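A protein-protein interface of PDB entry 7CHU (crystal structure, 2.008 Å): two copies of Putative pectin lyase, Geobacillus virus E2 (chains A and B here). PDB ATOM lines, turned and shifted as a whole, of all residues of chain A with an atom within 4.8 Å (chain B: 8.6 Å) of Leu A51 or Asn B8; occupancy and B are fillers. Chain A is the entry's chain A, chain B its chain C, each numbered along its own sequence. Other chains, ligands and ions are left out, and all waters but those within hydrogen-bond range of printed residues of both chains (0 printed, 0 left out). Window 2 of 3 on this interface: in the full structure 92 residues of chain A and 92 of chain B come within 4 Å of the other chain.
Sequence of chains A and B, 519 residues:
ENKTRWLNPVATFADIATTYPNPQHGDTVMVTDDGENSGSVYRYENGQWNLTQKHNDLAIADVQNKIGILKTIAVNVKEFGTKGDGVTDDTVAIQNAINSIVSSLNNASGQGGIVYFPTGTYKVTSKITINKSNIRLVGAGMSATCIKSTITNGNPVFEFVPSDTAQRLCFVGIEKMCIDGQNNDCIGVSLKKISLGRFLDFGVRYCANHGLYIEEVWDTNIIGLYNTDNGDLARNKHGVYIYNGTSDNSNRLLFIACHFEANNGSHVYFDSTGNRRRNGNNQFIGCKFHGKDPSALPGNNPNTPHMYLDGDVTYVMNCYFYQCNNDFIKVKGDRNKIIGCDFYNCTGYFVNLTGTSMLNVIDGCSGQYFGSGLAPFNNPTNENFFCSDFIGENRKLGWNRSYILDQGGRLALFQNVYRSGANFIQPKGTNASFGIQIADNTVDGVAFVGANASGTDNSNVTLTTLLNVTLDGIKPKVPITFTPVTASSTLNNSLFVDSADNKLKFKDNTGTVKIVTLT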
ATOM      1  N   SER A  40     -15.201  19.324 -16.333  1.00  0.00           N
ATOM      2  CA  SER A  40     -14.210  18.603 -17.116  1.00  0.00           C
ATOM      3  C   SER A  40     -14.613  17.144 -17.263  1.00  0.00           C
ATOM      4  O   SER A  40     -15.132  16.528 -16.325  1.00  0.00           O
ATOM      5  CB  SER A  40     -12.835  18.728 -16.458  1.00  0.00           C
ATOM      6  OG  SER A  40     -12.487  20.095 -16.288  1.00  0.00           O
ATOM      7  N   VAL A  41     -14.397  16.608 -18.464  1.00  0.00           N
ATOM      8  CA  VAL A  41     -14.768  15.246 -18.824  1.00  0.00           C
ATOM      9  C   VAL A  41     -13.483  14.513 -19.193  1.00  0.00           C
ATOM     10  O   VAL A  41     -12.702  14.996 -20.024  1.00  0.00           O
ATOM     11  CB  VAL A  41     -15.785  15.221 -19.979  1.00  0.00           C
ATOM     12  CG1 VAL A  41     -15.955  13.825 -20.537  1.00  0.00           C
ATOM     13  CG2 VAL A  41     -17.134  15.759 -19.510  1.00  0.00           C
ATOM     14  N   TYR A  42     -13.252  13.363 -18.564  1.00  0.00           N
ATOM     15  CA  TYR A  42     -12.020  12.615 -18.753  1.00  0.00           C
ATOM     16  C   TYR A  42     -12.348  11.269 -19.375  1.00  0.00           C
ATOM     17  O   TYR A  42     -13.368  10.649 -19.048  1.00  0.00           O
ATOM     18  CB  TYR A  42     -11.255  12.442 -17.423  1.00  0.00           C
ATOM     19  CG  TYR A  42     -10.831  13.765 -16.798  1.00  0.00           C
ATOM     20  CD1 TYR A  42      -9.584  14.330 -17.068  1.00  0.00           C
ATOM     21  CD2 TYR A  42     -11.688  14.455 -15.953  1.00  0.00           C
ATOM     22  CE1 TYR A  42      -9.211  15.546 -16.498  1.00  0.00           C
ATOM     23  CE2 TYR A  42     -11.325  15.660 -15.383  1.00  0.00           C
ATOM     24  CZ  TYR A  42     -10.092  16.205 -15.658  1.00  0.00           C
ATOM     25  OH  TYR A  42      -9.764  17.412 -15.078  1.00  0.00           O
ATOM     26  N   TRP A  49      -6.032   8.667 -17.661  1.00  0.00           N
ATOM     27  CA  TRP A  49      -7.239   9.471 -17.790  1.00  0.00           C
ATOM     28  C   TRP A  49      -6.875  10.747 -18.541  1.00  0.00           C
ATOM     29  O   TRP A  49      -6.004  11.504 -18.101  1.00  0.00           O
ATOM     30  CB  TRP A  49      -7.834   9.798 -16.421  1.00  0.00           C
ATOM     31  CG  TRP A  49      -8.496   8.638 -15.737  1.00  0.00           C
ATOM     32  CD1 TRP A  49      -7.977   7.868 -14.732  1.00  0.00           C
ATOM     33  CD2 TRP A  49      -9.808   8.121 -16.002  1.00  0.00           C
ATOM     34  NE1 TRP A  49      -8.883   6.904 -14.358  1.00  0.00           N
ATOM     35  CE2 TRP A  49     -10.014   7.036 -15.123  1.00  0.00           C
ATOM     36  CE3 TRP A  49     -10.829   8.469 -16.899  1.00  0.00           C
ATOM     37  CZ2 TRP A  49     -11.199   6.298 -15.112  1.00  0.00           C
ATOM     38  CZ3 TRP A  49     -12.009   7.732 -16.888  1.00  0.00           C
ATOM     39  CH2 TRP A  49     -12.180   6.656 -16.003  1.00  0.00           C
ATOM     40  N   ASN A  50      -7.525  10.982 -19.675  1.00  0.00           N
ATOM     41  CA  ASN A  50      -7.206  12.115 -20.534  1.00  0.00           C
ATOM     42  C   ASN A  50      -8.378  13.083 -20.555  1.00  0.00           C
ATOM     43  O   ASN A  50      -9.517  12.672 -20.800  1.00  0.00           O
ATOM     44  CB  ASN A  50      -6.887  11.658 -21.962  1.00  0.00           C
ATOM     45  CG  ASN A  50      -5.658  10.772 -22.032  1.00  0.00           C
ATOM     46  OD1 ASN A  50      -5.758   9.573 -22.304  1.00  0.00           O
ATOM     47  ND2 ASN A  50      -4.490  11.361 -21.795  1.00  0.00           N
ATOM     48  N   LEU A  51      -8.099  14.360 -20.306  1.00  0.00           N
ATOM     49  CA  LEU A  51      -9.119  15.388 -20.461  1.00  0.00           C
ATOM     50  C   LEU A  51      -9.498  15.504 -21.932  1.00  0.00           C
ATOM     51  O   LEU A  51      -8.646  15.793 -22.775  1.00  0.00           O
ATOM     52  CB  LEU A  51      -8.612  16.722 -19.924  1.00  0.00           C
ATOM     53  CG  LEU A  51      -9.606  17.887 -19.950  1.00  0.00           C
ATOM     54  CD1 LEU A  51     -10.784  17.591 -19.025  1.00  0.00           C
ATOM     55  CD2 LEU A  51      -8.928  19.184 -19.549  1.00  0.00           C
ATOM     56  N   THR A  52     -10.768  15.271 -22.247  1.00  0.00           N
ATOM     57  CA  THR A  52     -11.247  15.356 -23.625  1.00  0.00           C
ATOM     58  C   THR A  52     -12.299  16.432 -23.844  1.00  0.00           C
ATOM     59  O   THR A  52     -12.346  17.021 -24.932  1.00  0.00           O
ATOM     60  CB  THR A  52     -11.829  14.010 -24.084  1.00  0.00           C
ATOM     61  OG1 THR A  52     -13.069  13.759 -23.403  1.00  0.00           O
ATOM     62  CG2 THR A  52     -10.849  12.877 -23.808  1.00  0.00           C
ATOM     63  N   GLN A  53     -13.162  16.697 -22.863  1.00  0.00           N
ATOM     64  CA  GLN A  53     -14.256  17.640 -23.064  1.00  0.00           C
ATOM     65  C   GLN A  53     -14.434  18.477 -21.807  1.00  0.00           C
ATOM     66  O   GLN A  53     -13.959  18.120 -20.726  1.00  0.00           O
ATOM     67  CB  GLN A  53     -15.565  16.919 -23.436  1.00  0.00           C
ATOM     68  CG  GLN A  53     -15.431  15.939 -24.606  1.00  0.00           C
ATOM     69  CD  GLN A  53     -16.713  15.181 -24.914  1.00  0.00           C
ATOM     70  OE1 GLN A  53     -17.701  15.773 -25.327  1.00  0.00           O
ATOM     71  NE2 GLN A  53     -16.688  13.864 -24.744  1.00  0.00           N
ATOM     72  N   ARG B   5      -9.749  10.236 -32.183  1.00  0.00           N
ATOM     73  CA  ARG B   5      -8.660  10.370 -31.215  1.00  0.00           C
ATOM     74  C   ARG B   5      -8.811  11.712 -30.505  1.00  0.00           C
ATOM     75  O   ARG B   5      -8.421  12.754 -31.043  1.00  0.00           O
ATOM     76  CB  ARG B   5      -7.295  10.266 -31.892  1.00  0.00           C
ATOM     77  CG  ARG B   5      -7.085   8.988 -32.683  1.00  0.00           C
ATOM     78  CD  ARG B   5      -5.601   8.696 -32.919  1.00  0.00           C
ATOM     79  NE  ARG B   5      -5.391   7.989 -34.182  1.00  0.00           N
ATOM     80  CZ  ARG B   5      -5.590   6.685 -34.356  1.00  0.00           C
ATOM     81  NH1 ARG B   5      -6.002   5.924 -33.347  1.00  0.00           N
ATOM     82  NH2 ARG B   5      -5.377   6.137 -35.546  1.00  0.00           N
ATOM     83  N   TRP B   6      -9.349  11.688 -29.291  1.00  0.00           N
ATOM     84  CA  TRP B   6      -9.592  12.925 -28.570  1.00  0.00           C
ATOM     85  C   TRP B   6      -8.283  13.599 -28.190  1.00  0.00           C
ATOM     86  O   TRP B   6      -7.380  12.960 -27.646  1.00  0.00           O
ATOM     87  CB  TRP B   6     -10.417  12.647 -27.316  1.00  0.00           C
ATOM     88  CG  TRP B   6     -11.868  12.442 -27.583  1.00  0.00           C
ATOM     89  CD1 TRP B   6     -12.523  11.254 -27.720  1.00  0.00           C
ATOM     90  CD2 TRP B   6     -12.852  13.466 -27.750  1.00  0.00           C
ATOM     91  NE1 TRP B   6     -13.853  11.476 -27.959  1.00  0.00           N
ATOM     92  CE2 TRP B   6     -14.084  12.825 -27.985  1.00  0.00           C
ATOM     93  CE3 TRP B   6     -12.808  14.860 -27.726  1.00  0.00           C
ATOM     94  CZ2 TRP B   6     -15.265  13.525 -28.188  1.00  0.00           C
ATOM     95  CZ3 TRP B   6     -13.973  15.558 -27.932  1.00  0.00           C
ATOM     96  CH2 TRP B   6     -15.189  14.893 -28.162  1.00  0.00           C
ATOM     97  N   LEU B   7      -8.182  14.890 -28.469  1.00  0.00           N
ATOM     98  CA  LEU B   7      -7.105  15.707 -27.936  1.00  0.00           C
ATOM     99  C   LEU B   7      -7.620  16.509 -26.755  1.00  0.00           C
ATOM    100  O   LEU B   7      -8.826  16.628 -26.529  1.00  0.00           O
ATOM    101  CB  LEU B   7      -6.525  16.658 -28.984  1.00  0.00           C
ATOM    102  CG  LEU B   7      -5.854  16.056 -30.217  1.00  0.00           C
ATOM    103  CD1 LEU B   7      -4.936  14.884 -29.854  1.00  0.00           C
ATOM    104  CD2 LEU B   7      -6.901  15.646 -31.211  1.00  0.00           C
ATOM    105  N   ASN B   8      -6.687  17.053 -25.997  1.00  0.00           N
ATOM    106  CA  ASN B   8      -7.078  17.873 -24.871  1.00  0.00           C
ATOM    107  C   ASN B   8      -7.728  19.153 -25.390  1.00  0.00           C
ATOM    108  O   ASN B   8      -7.263  19.721 -26.385  1.00  0.00           O
ATOM    109  CB  ASN B   8      -5.865  18.172 -23.990  1.00  0.00           C
ATOM    110  CG  ASN B   8      -5.342  16.925 -23.284  1.00  0.00           C
ATOM    111  OD1 ASN B   8      -4.456  17.005 -22.431  1.00  0.00           O
ATOM    112  ND2 ASN B   8      -5.896  15.765 -23.634  1.00  0.00           N
ATOM    113  N   PRO B   9      -8.820  19.611 -24.776  1.00  0.00           N
ATOM    114  CA  PRO B   9      -9.519  20.788 -25.301  1.00  0.00           C
ATOM    115  C   PRO B   9      -8.648  22.034 -25.243  1.00  0.00           C
ATOM    116  O   PRO B   9      -7.662  22.113 -24.505  1.00  0.00           O
ATOM    117  CB  PRO B   9     -10.741  20.928 -24.381  1.00  0.00           C
ATOM    118  CG  PRO B   9     -10.829  19.640 -23.626  1.00  0.00           C
ATOM    119  CD  PRO B   9      -9.442  19.099 -23.544  1.00  0.00           C
ATOM    120  N   VAL B  10      -9.042  23.026 -26.041  1.00  0.00           N
ATOM    121  CA  VAL B  10      -8.384  24.322 -26.106  1.00  0.00           C
ATOM    122  C   VAL B  10      -9.449  25.395 -25.931  1.00  0.00           C
ATOM    123  O   VAL B  10     -10.643  25.149 -26.113  1.00  0.00           O
ATOM    124  CB  VAL B  10      -7.630  24.524 -27.438  1.00  0.00           C
ATOM    125  CG1 VAL B  10      -6.384  23.656 -27.490  1.00  0.00           C
ATOM    126  CG2 VAL B  10      -8.552  24.209 -28.610  1.00  0.00           C
ATOM    127  N   ALA B  11      -9.000  26.605 -25.591  1.00  0.00           N
ATOM    128  CA  ALA B  11      -9.932  27.694 -25.303  1.00  0.00           C
ATOM    129  C   ALA B  11     -10.665  28.151 -26.561  1.00  0.00           C
ATOM    130  O   ALA B  11     -11.900  28.179 -26.601  1.00  0.00           O
ATOM    131  CB  ALA B  11      -9.193  28.869 -24.652  1.00  0.00           C
ATOM    132  N   ASP B  15      -6.650  29.041 -31.056  1.00  0.00           N
ATOM    133  CA  ASP B  15      -5.621  28.320 -30.324  1.00  0.00           C
ATOM    134  C   ASP B  15      -5.273  26.984 -30.971  1.00  0.00           C
ATOM    135  O   ASP B  15      -4.188  26.459 -30.709  1.00  0.00           O
ATOM    136  CB  ASP B  15      -6.067  28.097 -28.873  1.00  0.00           C
ATOM    137  CG  ASP B  15      -6.142  29.397 -28.070  1.00  0.00           C
ATOM    138  OD1 ASP B  15      -5.245  30.258 -28.211  1.00  0.00           O
ATOM    139  OD2 ASP B  15      -7.101  29.558 -27.286  1.00  0.00           O
ATOM    140  N   ILE B  16      -6.150  26.430 -31.817  1.00  0.00           N
ATOM    141  CA  ILE B  16      -5.935  25.077 -32.335  1.00  0.00           C
ATOM    142  C   ILE B  16      -4.640  24.999 -33.134  1.00  0.00           C
ATOM    143  O   ILE B  16      -3.818  24.095 -32.922  1.00  0.00           O
ATOM    144  CB  ILE B  16      -7.135  24.611 -33.184  1.00  0.00           C
ATOM    145  CG1 ILE B  16      -8.414  24.563 -32.347  1.00  0.00           C
ATOM    146  CG2 ILE B  16      -6.854  23.232 -33.771  1.00  0.00           C
ATOM    147  CD1 ILE B  16      -9.482  23.640 -32.904  1.00  0.00           C
ATOM    148  N   THR B  19      -1.569  25.699 -30.633  1.00  0.00           N
ATOM    149  CA  THR B  19      -1.330  24.605 -29.704  1.00  0.00           C
ATOM    150  C   THR B  19      -1.027  23.300 -30.433  1.00  0.00           C
ATOM    151  O   THR B  19      -0.239  22.479 -29.948  1.00  0.00           O
ATOM    152  CB  THR B  19      -2.548  24.443 -28.807  1.00  0.00           C
ATOM    153  OG1 THR B  19      -3.736  24.388 -29.617  1.00  0.00           O
ATOM    154  CG2 THR B  19      -2.659  25.637 -27.857  1.00  0.00           C
ATOM    155  N   TYR B  20      -1.648  23.085 -31.599  1.00  0.00           N
ATOM    156  CA  TYR B  20      -1.485  21.871 -32.401  1.00  0.00           C
ATOM    157  C   TYR B  20      -1.034  22.287 -33.796  1.00  0.00           C
ATOM    158  O   TYR B  20      -1.863  22.392 -34.713  1.00  0.00           O
ATOM    159  CB  TYR B  20      -2.779  21.062 -32.489  1.00  0.00           C
ATOM    160  CG  TYR B  20      -3.337  20.582 -31.161  1.00  0.00           C
ATOM    161  CD1 TYR B  20      -3.416  19.228 -30.869  1.00  0.00           C
ATOM    162  CD2 TYR B  20      -3.809  21.487 -30.208  1.00  0.00           C
ATOM    163  CE1 TYR B  20      -3.929  18.789 -29.661  1.00  0.00           C
ATOM    164  CE2 TYR B  20      -4.324  21.057 -28.998  1.00  0.00           C
ATOM    165  CZ  TYR B  20      -4.385  19.706 -28.732  1.00  0.00           C
ATOM    166  OH  TYR B  20      -4.898  19.266 -27.535  1.00  0.00           O
ATOM    167  N   THR B  28      -9.433  14.989 -32.833  1.00  0.00           N
ATOM    168  CA  THR B  28     -10.682  15.622 -32.426  1.00  0.00           C
ATOM    169  C   THR B  28     -10.436  16.471 -31.191  1.00  0.00           C
ATOM    170  O   THR B  28      -9.904  15.974 -30.192  1.00  0.00           O
ATOM    171  CB  THR B  28     -11.759  14.575 -32.122  1.00  0.00           C
ATOM    172  OG1 THR B  28     -11.954  13.713 -33.255  1.00  0.00           O
ATOM    173  CG2 THR B  28     -13.064  15.252 -31.765  1.00  0.00           C
ATOM    174  N   VAL B  29     -10.837  17.739 -31.244  1.00  0.00           N
ATOM    175  CA  VAL B  29     -10.697  18.638 -30.103  1.00  0.00           C
ATOM    176  C   VAL B  29     -11.948  19.505 -29.984  1.00  0.00           C
ATOM    177  O   VAL B  29     -12.583  19.846 -30.989  1.00  0.00           O
ATOM    178  CB  VAL B  29      -9.408  19.486 -30.222  1.00  0.00           C
ATOM    179  CG1 VAL B  29      -9.506  20.465 -31.379  1.00  0.00           C
ATOM    180  CG2 VAL B  29      -9.097  20.208 -28.907  1.00  0.00           C
ATOM    181  N   MET B  30     -12.319  19.820 -28.742  1.00  0.00           N
ATOM    182  CA  MET B  30     -13.424  20.712 -28.420  1.00  0.00           C
ATOM    183  C   MET B  30     -12.856  22.069 -28.024  1.00  0.00           C
ATOM    184  O   MET B  30     -11.826  22.148 -27.349  1.00  0.00           O
ATOM    185  CB  MET B  30     -14.279  20.134 -27.276  1.00  0.00           C
ATOM    186  CG  MET B  30     -15.513  20.972 -26.856  1.00  0.00           C
ATOM    187  SD  MET B  30     -16.437  20.364 -25.393  1.00  0.00           S
ATOM    188  CE  MET B  30     -17.191  18.874 -25.995  1.00  0.00           C
ATOM    189  N   VAL B  31     -13.511  23.133 -28.461  1.00  0.00           N
ATOM    190  CA  VAL B  31     -13.187  24.472 -27.990  1.00  0.00           C
ATOM    191  C   VAL B  31     -14.122  24.797 -26.832  1.00  0.00           C
ATOM    192  O   VAL B  31     -15.335  24.579 -26.918  1.00  0.00           O
ATOM    193  CB  VAL B  31     -13.296  25.503 -29.128  1.00  0.00           C
ATOM    194  CG1 VAL B  31     -12.155  25.309 -30.117  1.00  0.00           C
ATOM    195  CG2 VAL B  31     -14.648  25.400 -29.851  1.00  0.00           C
ATOM    196  N   THR B  32     -13.559  25.298 -25.733  1.00  0.00           N
ATOM    197  CA  THR B  32     -14.306  25.403 -24.491  1.00  0.00           C
ATOM    198  C   THR B  32     -14.476  26.823 -23.969  1.00  0.00           C
ATOM    199  O   THR B  32     -15.302  27.028 -23.072  1.00  0.00           O
ATOM    200  CB  THR B  32     -13.639  24.554 -23.390  1.00  0.00           C
ATOM    201  OG1 THR B  32     -12.332  25.060 -23.123  1.00  0.00           O
ATOM    202  CG2 THR B  32     -13.508  23.101 -23.826  1.00  0.00           C
ATOM    203  N   TRP B  49      -9.215  21.310 -40.291  1.00  0.00           N
ATOM    204  CA  TRP B  49     -10.046  21.046 -39.124  1.00  0.00           C
ATOM    205  C   TRP B  49     -11.515  21.229 -39.500  1.00  0.00           C
ATOM    206  O   TRP B  49     -11.903  22.284 -40.007  1.00  0.00           O
ATOM    207  CB  TRP B  49      -9.661  21.983 -37.978  1.00  0.00           C
ATOM    208  CG  TRP B  49      -8.322  21.675 -37.358  1.00  0.00           C
ATOM    209  CD1 TRP B  49      -7.135  22.309 -37.603  1.00  0.00           C
ATOM    210  CD2 TRP B  49      -8.039  20.658 -36.389  1.00  0.00           C
ATOM    211  NE1 TRP B  49      -6.133  21.748 -36.845  1.00  0.00           N
ATOM    212  CE2 TRP B  49      -6.661  20.730 -36.094  1.00  0.00           C
ATOM    213  CE3 TRP B  49      -8.817  19.694 -35.740  1.00  0.00           C
ATOM    214  CZ2 TRP B  49      -6.048  19.876 -35.178  1.00  0.00           C
ATOM    215  CZ3 TRP B  49      -8.206  18.842 -34.837  1.00  0.00           C
ATOM    216  CH2 TRP B  49      -6.836  18.940 -34.563  1.00  0.00           C
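Among the printed residues, merely in contact across the chains: Gln A53 with Met B30 (3.2 Å), Thr A52 with Pro B9 (3.3 Å), Leu A51 with Pro B9 (3.5 Å), Thr A52 with Trp B6 (3.5 Å), Gln A53 with Trp B6 (3.6 Å), Gln A53 with Pro B9 (3.8 Å), Leu A51 with Leu B7 (3.8 Å) and Thr A52 with Leu B7 (3.9 Å).
The backbone carbonyl oxygen (O) of Gln A53 lies within hydrogen-bond range of the backbone NH (N) of Val A41, 2.8 Å away. The backbone carbonyl oxygen of Asn B8 is in hydrogen-bond range of the side-chain hydroxyl of Tyr B20 (2.7 Å). O of Val A41 lies within hydrogen-bond range of N of Thr A52, at 3.0 Å. N of Leu B7 sits at hydrogen-bond distance from O of Thr B28, at 2.7 Å. The backbone NH (N) of Val B10 sits at hydrogen-bond distance from the backbone carbonyl oxygen (O) of Met B30, at 3.2 Å.
ND2 of Asn B8 lies within hydrogen-bond range of O of Leu A51, at 2.9 Å.
Ser A40 touches none of the printed residues of chain B. Of chain B, only Leu B7 (3.8 Å), Asn B8 (2.9 Å) and Pro B9 (3.5 Å) come within 4 Å of Leu A51. Of the printed residues of chain B, Thr A52 touches Trp B6, Leu B7 and Pro B9. Printed residues of chain A within 4 Å of Pro B9: Leu A51, Thr A52 and Gln A53. Of the printed residues of chain A, Met B30 touches Gln A53 (3.2 Å). Thr B32 touches none of the printed residues of chain A. The nearest residue of chain A that does not touch Asn B8 is Asn A50 (4.5 Å).
Position printed for both chains: 49.
Printed residues of chain A that touch a printed residue of chain B: Leu A51, Thr A52 and Gln A53. Of the 17 printed residues of chain B, 5 touch a printed residue of chain A. Hydrophobic or aromatic side chains of chain B within 4 Å of the printed part of chain A: Trp B6, Pro B9 and Met B30. Along chain B the printed residues that touch a printed residue of chain A span positions 6 to 30. Among the printed residues, 9 pairs touch across the chains. Among the printed residues, no Asp or Glu carboxylate lies within 4 Å of a Lys or Arg side-chain nitrogen of the other chain.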
